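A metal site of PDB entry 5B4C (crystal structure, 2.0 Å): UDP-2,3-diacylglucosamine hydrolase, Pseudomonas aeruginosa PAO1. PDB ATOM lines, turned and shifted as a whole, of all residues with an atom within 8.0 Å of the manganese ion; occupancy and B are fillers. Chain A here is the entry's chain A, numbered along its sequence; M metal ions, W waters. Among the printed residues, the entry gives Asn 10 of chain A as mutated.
The backbone NH of Arg 80 lies within hydrogen-bond range of the side-chain carboxylate of Asp 41, 3.0 Å away.
The backbone NH (N) of Asn 10 lies within hydrogen-bond range of the backbone carbonyl oxygen (O) of Asp 41.
N of Asp 41 lies within hydrogen-bond range of OD1 of Asp 81 (3.0 Å).
O of His 114 lies within hydrogen-bond range of N of Gly 194, 2.8 Å away.
O of Leu 39 sits at hydrogen-bond distance from ND1 of His 114 (2.8 Å).
The side-chain carboxylate (OD2) of Asp 8 lies within hydrogen-bond range of the backbone NH (N) of His 195 (2.8 Å).
Of the 21 residues printed, 4 come within 4 Å of the manganese ion.
The manganese ion is bound by water W1 (2.1 Å), the side-chain amide oxygen of Asn 79 (2.1 Å), the side-chain carboxylate of Asp 41 (2.2 Å), a ring nitrogen (NE2) of His 114 (2.3 Å), water W2 (2.3 Å) and a ring nitrogen (ND1) of His 195 (2.3 Å).
The manganese ion has six donor atoms within binding distance.
Water W2 lies within hydrogen-bond range of O of His 195 (2.8 Å) and OD1 of Asp 8 (3.3 Å).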
ATOM      1  N   ASP A   8      30.754  30.726   7.686  1.00  0.00           N
ATOM      2  CA  ASP A   8      31.307  30.172   6.441  1.00  0.00           C
ATOM      3  C   ASP A   8      32.756  29.721   6.602  1.00  0.00           C
ATOM      4  O   ASP A   8      33.597  29.962   5.746  1.00  0.00           O
ATOM      5  CB  ASP A   8      31.168  31.171   5.305  1.00  0.00           C
ATOM      6  CG  ASP A   8      29.734  31.597   5.115  1.00  0.00           C
ATOM      7  OD1 ASP A   8      28.942  30.767   4.663  1.00  0.00           O
ATOM      8  OD2 ASP A   8      29.387  32.736   5.469  1.00  0.00           O
ATOM      9  N   ASN A  10      33.354  26.375   6.980  1.00  0.00           N
ATOM     10  CA  ASN A  10      33.328  25.098   6.267  1.00  0.00           C
ATOM     11  C   ASN A  10      34.413  24.160   6.780  1.00  0.00           C
ATOM     12  O   ASN A  10      35.161  23.532   5.999  1.00  0.00           O
ATOM     13  CB  ASN A  10      33.447  25.319   4.762  1.00  0.00           C
ATOM     14  CG  ASN A  10      32.267  26.064   4.213  1.00  0.00           C
ATOM     15  OD1 ASN A  10      31.181  25.495   4.065  1.00  0.00           O
ATOM     16  ND2 ASN A  10      32.437  27.341   3.975  1.00  0.00           N
ATOM     17  N   LEU A  39      27.445  32.384  12.368  1.00  0.00           N
ATOM     18  CA  LEU A  39      26.215  32.519  11.586  1.00  0.00           C
ATOM     19  C   LEU A  39      26.161  31.537  10.420  1.00  0.00           C
ATOM     20  O   LEU A  39      25.905  31.906   9.251  1.00  0.00           O
ATOM     21  CB  LEU A  39      26.047  33.964  11.129  1.00  0.00           C
ATOM     22  CG  LEU A  39      26.064  35.038  12.199  1.00  0.00           C
ATOM     23  CD1 LEU A  39      25.570  36.372  11.582  1.00  0.00           C
ATOM     24  CD2 LEU A  39      25.214  34.677  13.410  1.00  0.00           C
ATOM     25  N   GLY A  40      26.378  30.250  10.691  1.00  0.00           N
ATOM     26  CA  GLY A  40      26.094  29.202   9.718  1.00  0.00           C
ATOM     27  C   GLY A  40      27.273  28.779   8.852  1.00  0.00           C
ATOM     28  O   GLY A  40      28.262  29.494   8.675  1.00  0.00           O
ATOM     29  N   ASP A  41      27.139  27.568   8.301  1.00  0.00           N
ATOM     30  CA  ASP A  41      28.173  26.934   7.491  1.00  0.00           C
ATOM     31  C   ASP A  41      29.494  26.902   8.258  1.00  0.00           C
ATOM     32  O   ASP A  41      30.575  27.141   7.719  1.00  0.00           O
ATOM     33  CB  ASP A  41      28.352  27.621   6.119  1.00  0.00           C
ATOM     34  CG  ASP A  41      27.158  27.396   5.176  1.00  0.00           C
ATOM     35  OD1 ASP A  41      26.142  26.828   5.628  1.00  0.00           O
ATOM     36  OD2 ASP A  41      27.253  27.793   3.990  1.00  0.00           O
ATOM     37  N   PHE A  42      29.357  26.610   9.551  1.00  0.00           N
ATOM     38  CA  PHE A  42      30.469  26.358  10.451  1.00  0.00           C
ATOM     39  C   PHE A  42      31.229  25.096  10.076  1.00  0.00           C
ATOM     40  O   PHE A  42      32.470  25.101   9.989  1.00  0.00           O
ATOM     41  CB  PHE A  42      29.905  26.271  11.868  1.00  0.00           C
ATOM     42  CG  PHE A  42      30.964  26.105  12.959  1.00  0.00           C
ATOM     43  CD1 PHE A  42      32.062  26.939  13.037  1.00  0.00           C
ATOM     44  CD2 PHE A  42      30.797  25.153  13.943  1.00  0.00           C
ATOM     45  CE1 PHE A  42      33.005  26.782  14.084  1.00  0.00           C
ATOM     46  CE2 PHE A  42      31.740  25.017  14.978  1.00  0.00           C
ATOM     47  CZ  PHE A  42      32.827  25.820  15.018  1.00  0.00           C
ATOM     48  N   HIS A  77      22.474  27.762  12.473  1.00  0.00           N
ATOM     49  CA  HIS A  77      22.549  26.922  11.294  1.00  0.00           C
ATOM     50  C   HIS A  77      22.887  27.737  10.052  1.00  0.00           C
ATOM     51  O   HIS A  77      22.436  28.872   9.878  1.00  0.00           O
ATOM     52  CB  HIS A  77      21.193  26.250  11.036  1.00  0.00           C
ATOM     53  CG  HIS A  77      20.858  25.187  12.040  1.00  0.00           C
ATOM     54  ND1 HIS A  77      19.561  24.883  12.388  1.00  0.00           N
ATOM     55  CD2 HIS A  77      21.641  24.343  12.732  1.00  0.00           C
ATOM     56  CE1 HIS A  77      19.566  23.904  13.266  1.00  0.00           C
ATOM     57  NE2 HIS A  77      20.814  23.568  13.499  1.00  0.00           N
ATOM     58  N   GLY A  78      23.623  27.105   9.154  1.00  0.00           N
ATOM     59  CA  GLY A  78      23.653  27.473   7.755  1.00  0.00           C
ATOM     60  C   GLY A  78      22.990  26.392   6.926  1.00  0.00           C
ATOM     61  O   GLY A  78      22.458  25.413   7.443  1.00  0.00           O
ATOM     62  N   ASN A  79      23.032  26.583   5.594  1.00  0.00           N
ATOM     63  CA  ASN A  79      22.425  25.578   4.734  1.00  0.00           C
ATOM     64  C   ASN A  79      23.256  24.311   4.636  1.00  0.00           C
ATOM     65  O   ASN A  79      22.724  23.253   4.309  1.00  0.00           O
ATOM     66  CB  ASN A  79      22.185  26.116   3.295  1.00  0.00           C
ATOM     67  CG  ASN A  79      23.447  26.698   2.677  1.00  0.00           C
ATOM     68  OD1 ASN A  79      23.922  27.758   3.098  1.00  0.00           O
ATOM     69  ND2 ASN A  79      23.983  26.019   1.678  1.00  0.00           N
ATOM     70  N   ARG A  80      24.545  24.393   4.891  1.00  0.00           N
ATOM     71  CA  ARG A  80      25.351  23.191   4.825  1.00  0.00           C
ATOM     72  C   ARG A  80      25.306  22.376   6.102  1.00  0.00           C
ATOM     73  O   ARG A  80      25.563  21.173   6.061  1.00  0.00           O
ATOM     74  CB  ARG A  80      26.806  23.526   4.511  1.00  0.00           C
ATOM     75  CG  ARG A  80      26.960  24.343   3.248  1.00  0.00           C
ATOM     76  CD  ARG A  80      28.412  24.549   2.883  1.00  0.00           C
ATOM     77  NE  ARG A  80      28.983  23.368   2.242  1.00  0.00           N
ATOM     78  CZ  ARG A  80      28.882  23.104   0.940  1.00  0.00           C
ATOM     79  NH1 ARG A  80      29.420  21.996   0.457  1.00  0.00           N
ATOM     80  NH2 ARG A  80      28.238  23.946   0.136  1.00  0.00           N
ATOM     81  N   ASP A  81      24.975  22.989   7.225  1.00  0.00           N
ATOM     82  CA  ASP A  81      25.089  22.303   8.497  1.00  0.00           C
ATOM     83  C   ASP A  81      23.822  22.506   9.303  1.00  0.00           C
ATOM     84  O   ASP A  81      23.854  22.585  10.533  1.00  0.00           O
ATOM     85  CB  ASP A  81      26.338  22.749   9.250  1.00  0.00           C
ATOM     86  CG  ASP A  81      26.425  24.271   9.478  1.00  0.00           C
ATOM     87  OD1 ASP A  81      25.582  25.066   8.985  1.00  0.00           O
ATOM     88  OD2 ASP A  81      27.401  24.672  10.167  1.00  0.00           O
ATOM     89  N   HIS A 114      21.875  33.393   8.462  1.00  0.00           N
ATOM     90  CA  HIS A 114      22.937  32.881   7.611  1.00  0.00           C
ATOM     91  C   HIS A 114      23.019  33.655   6.296  1.00  0.00           C
ATOM     92  O   HIS A 114      24.113  33.974   5.825  1.00  0.00           O
ATOM     93  CB  HIS A 114      22.762  31.384   7.336  1.00  0.00           C
ATOM     94  CG  HIS A 114      23.815  30.812   6.436  1.00  0.00           C
ATOM     95  ND1 HIS A 114      25.154  30.849   6.746  1.00  0.00           N
ATOM     96  CD2 HIS A 114      23.735  30.197   5.225  1.00  0.00           C
ATOM     97  CE1 HIS A 114      25.851  30.297   5.764  1.00  0.00           C
ATOM     98  NE2 HIS A 114      25.018  29.885   4.828  1.00  0.00           N
ATOM     99  N   GLY A 115      21.864  33.959   5.683  1.00  0.00           N
ATOM    100  CA  GLY A 115      21.792  34.783   4.475  1.00  0.00           C
ATOM    101  C   GLY A 115      21.219  34.100   3.252  1.00  0.00           C
ATOM    102  O   GLY A 115      20.736  34.780   2.341  1.00  0.00           O
ATOM    103  N   ASP A 116      21.277  32.763   3.180  1.00  0.00           N
ATOM    104  CA  ASP A 116      20.813  32.105   1.959  1.00  0.00           C
ATOM    105  C   ASP A 116      19.309  32.268   1.768  1.00  0.00           C
ATOM    106  O   ASP A 116      18.834  32.258   0.631  1.00  0.00           O
ATOM    107  CB  ASP A 116      21.219  30.622   1.978  1.00  0.00           C
ATOM    108  CG  ASP A 116      20.483  29.853   3.068  1.00  0.00           C
ATOM    109  OD1 ASP A 116      20.546  30.273   4.238  1.00  0.00           O
ATOM    110  OD2 ASP A 116      19.829  28.850   2.733  1.00  0.00           O
ATOM    111  N   TYR A 125      17.583  26.466  -6.082  1.00  0.00           N
ATOM    112  CA  TYR A 125      18.064  26.418  -4.712  1.00  0.00           C
ATOM    113  C   TYR A 125      16.915  26.593  -3.729  1.00  0.00           C
ATOM    114  O   TYR A 125      16.838  25.874  -2.719  1.00  0.00           O
ATOM    115  CB  TYR A 125      19.132  27.478  -4.459  1.00  0.00           C
ATOM    116  CG  TYR A 125      19.528  27.436  -3.003  1.00  0.00           C
ATOM    117  CD1 TYR A 125      20.373  26.447  -2.515  1.00  0.00           C
ATOM    118  CD2 TYR A 125      18.995  28.330  -2.113  1.00  0.00           C
ATOM    119  CE1 TYR A 125      20.709  26.390  -1.162  1.00  0.00           C
ATOM    120  CE2 TYR A 125      19.306  28.287  -0.759  1.00  0.00           C
ATOM    121  CZ  TYR A 125      20.157  27.311  -0.297  1.00  0.00           C
ATOM    122  OH  TYR A 125      20.445  27.264   1.056  1.00  0.00           O
ATOM    123  N   ARG A 133      13.896  22.078   4.689  1.00  0.00           N
ATOM    124  CA  ARG A 133      13.417  22.626   5.965  1.00  0.00           C
ATOM    125  C   ARG A 133      11.980  22.336   6.269  1.00  0.00           C
ATOM    126  O   ARG A 133      11.511  22.769   7.321  1.00  0.00           O
ATOM    127  CB  ARG A 133      13.580  24.147   6.022  1.00  0.00           C
ATOM    128  CG  ARG A 133      14.925  24.609   5.624  1.00  0.00           C
ATOM    129  CD  ARG A 133      16.084  23.851   6.284  1.00  0.00           C
ATOM    130  NE  ARG A 133      17.304  24.409   5.731  1.00  0.00           N
ATOM    131  CZ  ARG A 133      18.025  25.369   6.292  1.00  0.00           C
ATOM    132  NH1 ARG A 133      19.078  25.815   5.647  1.00  0.00           N
ATOM    133  NH2 ARG A 133      17.711  25.856   7.500  1.00  0.00           N
ATOM    134  N   ILE A 171      27.667  31.294  -6.279  1.00  0.00           N
ATOM    135  CA  ILE A 171      26.752  31.563  -5.169  1.00  0.00           C
ATOM    136  C   ILE A 171      25.946  32.808  -5.540  1.00  0.00           C
ATOM    137  O   ILE A 171      26.500  33.913  -5.627  1.00  0.00           O
ATOM    138  CB  ILE A 171      27.497  31.751  -3.836  1.00  0.00           C
ATOM    139  CG1 ILE A 171      28.324  30.500  -3.475  1.00  0.00           C
ATOM    140  CG2 ILE A 171      26.491  32.060  -2.705  1.00  0.00           C
ATOM    141  CD1 ILE A 171      29.247  30.716  -2.253  1.00  0.00           C
ATOM    142  N   GLY A 194      25.995  35.946   6.593  1.00  0.00           N
ATOM    143  CA  GLY A 194      27.088  35.352   5.831  1.00  0.00           C
ATOM    144  C   GLY A 194      26.617  34.814   4.498  1.00  0.00           C
ATOM    145  O   GLY A 194      25.896  35.482   3.726  1.00  0.00           O
ATOM    146  N   HIS A 195      27.047  33.585   4.216  1.00  0.00           N
ATOM    147  CA  HIS A 195      26.621  32.753   3.094  1.00  0.00           C
ATOM    148  C   HIS A 195      27.136  33.206   1.722  1.00  0.00           C
ATOM    149  O   HIS A 195      27.549  32.350   0.934  1.00  0.00           O
ATOM    150  CB  HIS A 195      25.091  32.634   3.026  1.00  0.00           C
ATOM    151  CG  HIS A 195      24.611  31.922   1.792  1.00  0.00           C
ATOM    152  ND1 HIS A 195      24.723  30.552   1.628  1.00  0.00           N
ATOM    153  CD2 HIS A 195      24.072  32.392   0.637  1.00  0.00           C
ATOM    154  CE1 HIS A 195      24.263  30.210   0.439  1.00  0.00           C
ATOM    155  NE2 HIS A 195      23.849  31.306  -0.187  1.00  0.00           N
ATOM    156  N   THR A 196      27.061  34.498   1.391  1.00  0.00           N
ATOM    157  CA  THR A 196      27.327  34.937   0.019  1.00  0.00           C
ATOM    158  C   THR A 196      28.812  35.054  -0.303  1.00  0.00           C
ATOM    159  O   THR A 196      29.155  35.260  -1.482  1.00  0.00           O
ATOM    160  CB  THR A 196      26.663  36.278  -0.246  1.00  0.00           C
ATOM    161  OG1 THR A 196      27.204  37.245   0.647  1.00  0.00           O
ATOM    162  CG2 THR A 196      25.156  36.181   0.018  1.00  0.00           C
ATOM    163  N   HIS A 197      29.694  34.929   0.684  1.00  0.00           N
ATOM    164  CA  HIS A 197      31.148  34.952   0.436  1.00  0.00           C
ATOM    165  C   HIS A 197      31.589  36.286  -0.172  1.00  0.00           C
ATOM    166  O   HIS A 197      32.541  36.350  -0.943  1.00  0.00           O
ATOM    167  CB  HIS A 197      31.578  33.801  -0.472  1.00  0.00           C
ATOM    168  CG  HIS A 197      31.412  32.444   0.146  1.00  0.00           C
ATOM    169  ND1 HIS A 197      31.957  31.314  -0.429  1.00  0.00           N
ATOM    170  CD2 HIS A 197      30.760  32.021   1.262  1.00  0.00           C
ATOM    171  CE1 HIS A 197      31.647  30.255   0.306  1.00  0.00           C
ATOM    172  NE2 HIS A 197      30.933  30.657   1.335  1.00  0.00           N
HETATM  173 MN    MN M   1      25.726  28.891   2.908  1.00  0.00          MN
HETATM  174  O   HOH W   1      26.248  27.712   1.276  1.00  0.00           O
HETATM  175  O   HOH W   2      27.573  29.711   1.816  1.00  0.00           O
